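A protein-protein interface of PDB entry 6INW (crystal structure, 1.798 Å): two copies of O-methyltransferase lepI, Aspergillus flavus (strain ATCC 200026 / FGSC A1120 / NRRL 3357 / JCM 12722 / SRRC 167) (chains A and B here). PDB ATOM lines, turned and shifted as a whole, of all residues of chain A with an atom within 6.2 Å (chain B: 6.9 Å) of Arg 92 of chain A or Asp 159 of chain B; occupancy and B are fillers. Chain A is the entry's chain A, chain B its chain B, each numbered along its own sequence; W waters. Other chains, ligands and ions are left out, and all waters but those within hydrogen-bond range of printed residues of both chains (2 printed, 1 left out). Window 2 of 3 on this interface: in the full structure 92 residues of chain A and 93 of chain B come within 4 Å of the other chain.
The backbone carbonyl oxygen of Ala 85 of chain A sits at hydrogen-bond distance from the backbone NH of Cys 90 of chain A, 3.0 Å away. The side-chain carboxylate (OD2) of Asp 86 of chain A lies within salt-bridge range of the guanidinium group (NH2) of Arg 92 of chain A (2.9 Å). OE1 of Glu 82 of chain A lies within salt-bridge range of NH2 of Arg 92 of chain A, 2.8 Å away. The backbone carbonyl oxygen (O) of Leu 152 of chain B sits at hydrogen-bond distance from the backbone NH (N) of Tyr 157 of chain B.
Glu 82 of chain A touches none of the printed residues of chain B. Of the printed residues of chain B, Cys 90 of chain A touches Tyr 157 (3.9 Å). Of the printed residues of chain B, Gly 91 of chain A touches Tyr 157 (3.1 Å) and Asp 159 (3.4 Å). Arg 92 of chain A touches just one residue of chain B: Asp 159 (3.8 Å). Of the printed residues of chain B, Leu 94 of chain A touches Leu 152, Tyr 157, Pro 158, Asp 159 and Met 346. Lys 156 of chain B touches none of the printed residues of chain A. Of chain A, only Gly 91, Arg 92, Glu 93 and Leu 94 come within 4 Å of Asp 159 of chain B. Printed residues of chain A within 4 Å of Met 346 of chain B: Leu 94 and Arg 97. The nearest residue of chain B that does not touch Arg 92 of chain A is Tyr 157 of chain B (6.0 Å). The nearest residue of chain A that does not touch Asp 159 of chain B is Met 95 of chain A (5.1 Å). The nearest printed residue of chain A that does not touch Leu 152 of chain B is Cys 90 of chain A (6.9 Å).
No position is printed for both chains.
Of the 10 printed residues of chain B, 5 touch a printed residue of chain A. Printed residues of chain B that touch a printed residue of chain A: Leu 152, Tyr 157, Pro 158, Asp 159 and Met 346. Hydrophobic or aromatic side chains of chain B within 4 Å of the printed part of chain A: Leu 152, Tyr 157 and Met 346. Of the 12 printed residues of chain A, 6 touch a printed residue of chain B. Printed residues of chain A that touch a printed residue of chain B: Cys 90, Gly 91, Arg 92, Glu 93, Leu 94 and Arg 97. Among the printed residues, no Asp or Glu carboxylate lies within 4 Å of a Lys or Arg side-chain nitrogen of the other chain.
Water W1 lies within hydrogen-bond range of OD2 of Asp 159 of chain B (2.6 Å) and N of Glu 93 of chain A (3.2 Å). Water W2 lies within hydrogen-bond range of O of Ile 160 of chain B (2.6 Å) and NH1 of Arg 97 of chain A (2.8 Å).
The side-chain carboxylate (OD1) of Asp 159 of chain B sits at hydrogen-bond distance from the backbone NH (N) of Leu 94 of chain A. N of Glu 93 of chain A sits at hydrogen-bond distance from OD1 of Asp 159 of chain B, at 3.4 Å. NH1 of Arg 97 of chain A is in hydrogen-bond range of SD of Met 346 of chain B. The backbone NH (N) of Gly 91 of chain A is in hydrogen-bond range of the backbone carbonyl oxygen (O) of Tyr 157 of chain B (3.1 Å).
SG of Cys 90 of chain A touches CB of Tyr 157 of chain B, 3.9 Å away. Asp 159 of chain B touches Gly 91 of chain A. Arg 92 of chain A touches Asp 159 of chain B. Leu 94 of chain A touches Leu 152 of chain B (CD2 to CD2, 3.98 Å). Leu 94 of chain A touches Tyr 157 of chain B. Pro 158 of chain B touches Leu 94 of chain A (O to CD2, 3.5 Å). Met 346 of chain B touches Leu 94 of chain A.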
ATOM      1  N   ALA A  81      19.724  17.333 -21.325  1.00  0.00           N
ATOM      2  CA  ALA A  81      18.563  16.480 -21.562  1.00  0.00           C
ATOM      3  C   ALA A  81      17.586  17.141 -22.528  1.00  0.00           C
ATOM      4  O   ALA A  81      16.994  16.470 -23.380  1.00  0.00           O
ATOM      5  CB  ALA A  81      17.875  16.154 -20.236  1.00  0.00           C
ATOM      6  N   GLU A  82      17.404  18.457 -22.402  1.00  0.00           N
ATOM      7  CA  GLU A  82      16.547  19.202 -23.322  1.00  0.00           C
ATOM      8  C   GLU A  82      17.028  19.068 -24.763  1.00  0.00           C
ATOM      9  O   GLU A  82      16.234  18.803 -25.676  1.00  0.00           O
ATOM     10  CB  GLU A  82      16.505  20.668 -22.881  1.00  0.00           C
ATOM     11  CG  GLU A  82      15.704  21.598 -23.772  1.00  0.00           C
ATOM     12  CD  GLU A  82      15.690  23.032 -23.252  1.00  0.00           C
ATOM     13  OE1 GLU A  82      14.841  23.825 -23.711  1.00  0.00           O
ATOM     14  OE2 GLU A  82      16.531  23.368 -22.391  1.00  0.00           O
ATOM     15  N   ALA A  85      16.445  15.493 -26.011  1.00  0.00           N
ATOM     16  CA  ALA A  85      15.026  15.242 -26.233  1.00  0.00           C
ATOM     17  C   ALA A  85      14.556  15.886 -27.527  1.00  0.00           C
ATOM     18  O   ALA A  85      13.898  15.242 -28.353  1.00  0.00           O
ATOM     19  CB  ALA A  85      14.211  15.764 -25.049  1.00  0.00           C
ATOM     20  N   ASP A  86      14.897  17.160 -27.727  1.00  0.00           N
ATOM     21  CA  ASP A  86      14.453  17.849 -28.933  1.00  0.00           C
ATOM     22  C   ASP A  86      15.070  17.231 -30.181  1.00  0.00           C
ATOM     23  O   ASP A  86      14.391  17.083 -31.203  1.00  0.00           O
ATOM     24  CB  ASP A  86      14.784  19.337 -28.842  1.00  0.00           C
ATOM     25  CG  ASP A  86      14.073  20.020 -27.690  1.00  0.00           C
ATOM     26  OD1 ASP A  86      13.155  19.404 -27.102  1.00  0.00           O
ATOM     27  OD2 ASP A  86      14.438  21.171 -27.370  1.00  0.00           O
ATOM     28  N   CYS A  90      11.856  12.998 -28.395  1.00  0.00           N
ATOM     29  CA  CYS A  90      11.419  12.360 -27.165  1.00  0.00           C
ATOM     30  C   CYS A  90      10.879  13.425 -26.224  1.00  0.00           C
ATOM     31  O   CYS A  90      11.313  14.579 -26.260  1.00  0.00           O
ATOM     32  CB  CYS A  90      12.575  11.597 -26.506  1.00  0.00           C
ATOM     33  SG  CYS A  90      12.156  10.677 -25.005  1.00  0.00           S
ATOM     34  N   GLY A  91       9.923  13.033 -25.388  1.00  0.00           N
ATOM     35  CA  GLY A  91       9.434  13.949 -24.372  1.00  0.00           C
ATOM     36  C   GLY A  91      10.556  14.368 -23.439  1.00  0.00           C
ATOM     37  O   GLY A  91      11.415  13.565 -23.070  1.00  0.00           O
ATOM     38  N   ARG A  92      10.550  15.648 -23.060  1.00  0.00           N
ATOM     39  CA  ARG A  92      11.664  16.184 -22.281  1.00  0.00           C
ATOM     40  C   ARG A  92      11.760  15.523 -20.911  1.00  0.00           C
ATOM     41  O   ARG A  92      12.855  15.167 -20.459  1.00  0.00           O
ATOM     42  CB  ARG A  92      11.522  17.698 -22.141  1.00  0.00           C
ATOM     43  CG  ARG A  92      11.849  18.453 -23.418  1.00  0.00           C
ATOM     44  CD  ARG A  92      11.637  19.943 -23.249  1.00  0.00           C
ATOM     45  NE  ARG A  92      12.220  20.705 -24.349  1.00  0.00           N
ATOM     46  CZ  ARG A  92      12.405  22.019 -24.329  1.00  0.00           C
ATOM     47  NH1 ARG A  92      12.059  22.722 -23.258  1.00  0.00           N
ATOM     48  NH2 ARG A  92      12.943  22.633 -25.375  1.00  0.00           N
ATOM     49  N   GLU A  93      10.619  15.342 -20.243  1.00  0.00           N
ATOM     50  CA  GLU A  93      10.597  14.674 -18.945  1.00  0.00           C
ATOM     51  C   GLU A  93      11.034  13.219 -19.066  1.00  0.00           C
ATOM     52  O   GLU A  93      11.853  12.727 -18.274  1.00  0.00           O
ATOM     53  CB  GLU A  93       9.188  14.770 -18.358  1.00  0.00           C
ATOM     54  CG  GLU A  93       8.994  14.065 -17.031  1.00  0.00           C
ATOM     55  CD  GLU A  93       9.442  14.901 -15.856  1.00  0.00           C
ATOM     56  OE1 GLU A  93       8.586  15.225 -15.005  1.00  0.00           O
ATOM     57  OE2 GLU A  93      10.645  15.226 -15.780  1.00  0.00           O
ATOM     58  N   LEU A  94      10.467  12.506 -20.044  1.00  0.00           N
ATOM     59  CA  LEU A  94      10.861  11.123 -20.280  1.00  0.00           C
ATOM     60  C   LEU A  94      12.348  11.023 -20.584  1.00  0.00           C
ATOM     61  O   LEU A  94      13.035  10.139 -20.061  1.00  0.00           O
ATOM     62  CB  LEU A  94      10.034  10.531 -21.425  1.00  0.00           C
ATOM     63  CG  LEU A  94      10.425   9.145 -21.940  1.00  0.00           C
ATOM     64  CD1 LEU A  94      10.220   8.091 -20.860  1.00  0.00           C
ATOM     65  CD2 LEU A  94       9.616   8.808 -23.182  1.00  0.00           C
ATOM     66  N   MET A  95      12.862  11.922 -21.419  1.00  0.00           N
ATOM     67  CA  MET A  95      14.274  11.904 -21.785  1.00  0.00           C
ATOM     68  C   MET A  95      15.158  12.137 -20.564  1.00  0.00           C
ATOM     69  O   MET A  95      16.162  11.452 -20.379  1.00  0.00           O
ATOM     70  CB  MET A  95      14.562  12.956 -22.857  1.00  0.00           C
ATOM     71  CG  MET A  95      16.028  13.091 -23.231  1.00  0.00           C
ATOM     72  SD  MET A  95      16.746  11.471 -24.022  1.00  0.00           S
ATOM     73  CE  MET A  95      16.040  11.664 -25.811  1.00  0.00           C
ATOM     74  N   SER A  96      14.773  13.105 -19.727  1.00  0.00           N
ATOM     75  CA  SER A  96      15.550  13.392 -18.525  1.00  0.00           C
ATOM     76  C   SER A  96      15.574  12.196 -17.581  1.00  0.00           C
ATOM     77  O   SER A  96      16.627  11.850 -17.029  1.00  0.00           O
ATOM     78  CB  SER A  96      14.982  14.620 -17.817  1.00  0.00           C
ATOM     79  OG  SER A  96      15.662  14.851 -16.597  1.00  0.00           O
ATOM     80  N   ARG A  97      14.427  11.544 -17.386  1.00  0.00           N
ATOM     81  CA  ARG A  97      14.393  10.385 -16.496  1.00  0.00           C
ATOM     82  C   ARG A  97      15.190   9.217 -17.069  1.00  0.00           C
ATOM     83  O   ARG A  97      15.915   8.525 -16.335  1.00  0.00           O
ATOM     84  CB  ARG A  97      12.946   9.981 -16.228  1.00  0.00           C
ATOM     85  CG  ARG A  97      12.162  11.055 -15.487  1.00  0.00           C
ATOM     86  CD  ARG A  97      10.672  10.786 -15.536  1.00  0.00           C
ATOM     87  NE  ARG A  97      10.299   9.702 -14.636  1.00  0.00           N
ATOM     88  CZ  ARG A  97       9.053   9.285 -14.452  1.00  0.00           C
ATOM     89  NH1 ARG A  97       8.057   9.860 -15.112  1.00  0.00           N
ATOM     90  NH2 ARG A  97       8.807   8.294 -13.610  1.00  0.00           N
ATOM     91  N   LEU B 152       6.319   3.044 -25.665  1.00  0.00           N
ATOM     92  CA  LEU B 152       6.847   4.384 -25.912  1.00  0.00           C
ATOM     93  C   LEU B 152       6.989   4.652 -27.403  1.00  0.00           C
ATOM     94  O   LEU B 152       6.742   5.775 -27.861  1.00  0.00           O
ATOM     95  CB  LEU B 152       8.191   4.567 -25.204  1.00  0.00           C
ATOM     96  CG  LEU B 152       8.166   4.497 -23.674  1.00  0.00           C
ATOM     97  CD1 LEU B 152       9.579   4.581 -23.107  1.00  0.00           C
ATOM     98  CD2 LEU B 152       7.278   5.584 -23.077  1.00  0.00           C
ATOM     99  N   LYS B 156       4.990   7.677 -29.580  1.00  0.00           N
ATOM    100  CA  LYS B 156       5.947   8.740 -29.892  1.00  0.00           C
ATOM    101  C   LYS B 156       6.520   9.358 -28.620  1.00  0.00           C
ATOM    102  O   LYS B 156       6.646  10.579 -28.496  1.00  0.00           O
ATOM    103  CB  LYS B 156       5.308   9.807 -30.784  1.00  0.00           C
ATOM    104  CG  LYS B 156       4.464   9.240 -31.917  1.00  0.00           C
ATOM    105  CD  LYS B 156       5.271   9.122 -33.198  1.00  0.00           C
ATOM    106  CE  LYS B 156       5.556  10.491 -33.799  1.00  0.00           C
ATOM    107  NZ  LYS B 156       6.839  10.512 -34.558  1.00  0.00           N
ATOM    108  N   TYR B 157       6.853   8.496 -27.659  1.00  0.00           N
ATOM    109  CA  TYR B 157       7.647   8.839 -26.484  1.00  0.00           C
ATOM    110  C   TYR B 157       7.005   9.964 -25.682  1.00  0.00           C
ATOM    111  O   TYR B 157       7.563  11.065 -25.590  1.00  0.00           O
ATOM    112  CB  TYR B 157       9.071   9.188 -26.919  1.00  0.00           C
ATOM    113  CG  TYR B 157       9.706   8.018 -27.631  1.00  0.00           C
ATOM    114  CD1 TYR B 157      10.342   7.012 -26.914  1.00  0.00           C
ATOM    115  CD2 TYR B 157       9.610   7.881 -29.010  1.00  0.00           C
ATOM    116  CE1 TYR B 157      10.895   5.919 -27.554  1.00  0.00           C
ATOM    117  CE2 TYR B 157      10.162   6.790 -29.659  1.00  0.00           C
ATOM    118  CZ  TYR B 157      10.801   5.814 -28.926  1.00  0.00           C
ATOM    119  OH  TYR B 157      11.351   4.729 -29.564  1.00  0.00           O
ATOM    120  N   PRO B 158       5.846   9.721 -25.079  1.00  0.00           N
ATOM    121  CA  PRO B 158       5.192  10.761 -24.286  1.00  0.00           C
ATOM    122  C   PRO B 158       5.729  10.801 -22.866  1.00  0.00           C
ATOM    123  O   PRO B 158       6.354   9.857 -22.377  1.00  0.00           O
ATOM    124  CB  PRO B 158       3.726  10.326 -24.298  1.00  0.00           C
ATOM    125  CG  PRO B 158       3.815   8.825 -24.290  1.00  0.00           C
ATOM    126  CD  PRO B 158       5.063   8.471 -25.090  1.00  0.00           C
ATOM    127  N   ASP B 159       5.478  11.926 -22.205  1.00  0.00           N
ATOM    128  CA  ASP B 159       5.688  12.018 -20.767  1.00  0.00           C
ATOM    129  C   ASP B 159       4.523  11.327 -20.066  1.00  0.00           C
ATOM    130  O   ASP B 159       3.376  11.769 -20.180  1.00  0.00           O
ATOM    131  CB  ASP B 159       5.799  13.479 -20.332  1.00  0.00           C
ATOM    132  CG  ASP B 159       6.993  14.190 -20.954  1.00  0.00           C
ATOM    133  OD1 ASP B 159       8.001  13.519 -21.267  1.00  0.00           O
ATOM    134  OD2 ASP B 159       6.925  15.425 -21.127  1.00  0.00           O
ATOM    135  N   ILE B 160       4.814  10.254 -19.336  1.00  0.00           N
ATOM    136  CA  ILE B 160       3.765   9.442 -18.724  1.00  0.00           C
ATOM    137  C   ILE B 160       3.347  10.087 -17.411  1.00  0.00           C
ATOM    138  O   ILE B 160       4.174  10.301 -16.519  1.00  0.00           O
ATOM    139  CB  ILE B 160       4.239   8.001 -18.502  1.00  0.00           C
ATOM    140  CG1 ILE B 160       4.531   7.325 -19.846  1.00  0.00           C
ATOM    141  CG2 ILE B 160       3.198   7.220 -17.718  1.00  0.00           C
ATOM    142  CD1 ILE B 160       5.219   5.985 -19.720  1.00  0.00           C
ATOM    143  N   VAL B 161       2.051  10.402 -17.288  1.00  0.00           N
ATOM    144  CA  VAL B 161       1.526  11.088 -16.118  1.00  0.00           C
ATOM    145  C   VAL B 161       0.233  10.482 -15.591  1.00  0.00           C
ATOM    146  O   VAL B 161      -0.313  10.980 -14.608  1.00  0.00           O
ATOM    147  CB  VAL B 161       1.317  12.591 -16.403  1.00  0.00           C
ATOM    148  CG1 VAL B 161       2.650  13.290 -16.614  1.00  0.00           C
ATOM    149  CG2 VAL B 161       0.411  12.772 -17.616  1.00  0.00           C
ATOM    150  N   ASP B 162      -0.282   9.417 -16.205  1.00  0.00           N
ATOM    151  CA  ASP B 162      -1.554   8.838 -15.783  1.00  0.00           C
ATOM    152  C   ASP B 162      -1.403   7.347 -15.523  1.00  0.00           C
ATOM    153  O   ASP B 162      -0.867   6.614 -16.361  1.00  0.00           O
ATOM    154  CB  ASP B 162      -2.656   9.087 -16.810  1.00  0.00           C
ATOM    155  CG  ASP B 162      -4.049   8.872 -16.238  1.00  0.00           C
ATOM    156  OD1 ASP B 162      -4.414   7.706 -15.960  1.00  0.00           O
ATOM    157  OD2 ASP B 162      -4.773   9.874 -16.049  1.00  0.00           O
ATOM    158  N   ASP B 165      -2.865   5.003 -18.201  1.00  0.00           N
ATOM    159  CA  ASP B 165      -2.337   5.103 -19.556  1.00  0.00           C
ATOM    160  C   ASP B 165      -0.807   5.005 -19.520  1.00  0.00           C
ATOM    161  O   ASP B 165      -0.080   5.970 -19.750  1.00  0.00           O
ATOM    162  CB  ASP B 165      -2.792   6.400 -20.228  1.00  0.00           C
ATOM    163  CG  ASP B 165      -2.434   6.448 -21.698  1.00  0.00           C
ATOM    164  OD1 ASP B 165      -2.207   5.373 -22.292  1.00  0.00           O
ATOM    165  OD2 ASP B 165      -2.379   7.563 -22.261  1.00  0.00           O
ATOM    166  N   MET B 346       7.181   4.369 -13.103  1.00  0.00           N
ATOM    167  CA  MET B 346       6.621   5.034 -14.269  1.00  0.00           C
ATOM    168  C   MET B 346       5.892   4.027 -15.148  1.00  0.00           C
ATOM    169  O   MET B 346       4.772   4.274 -15.603  1.00  0.00           O
ATOM    170  CB  MET B 346       7.711   5.729 -15.075  1.00  0.00           C
ATOM    171  CG  MET B 346       7.205   6.355 -16.355  1.00  0.00           C
ATOM    172  SD  MET B 346       8.670   6.955 -17.476  1.00  0.00           S
ATOM    173  CE  MET B 346       9.228   5.234 -18.171  1.00  0.00           C
HETATM  174  O   HOH W   1       8.266  17.547 -20.386  1.00  0.00           O
HETATM  175  O   HOH W   2       5.521   8.737 -14.895  1.00  0.00           O
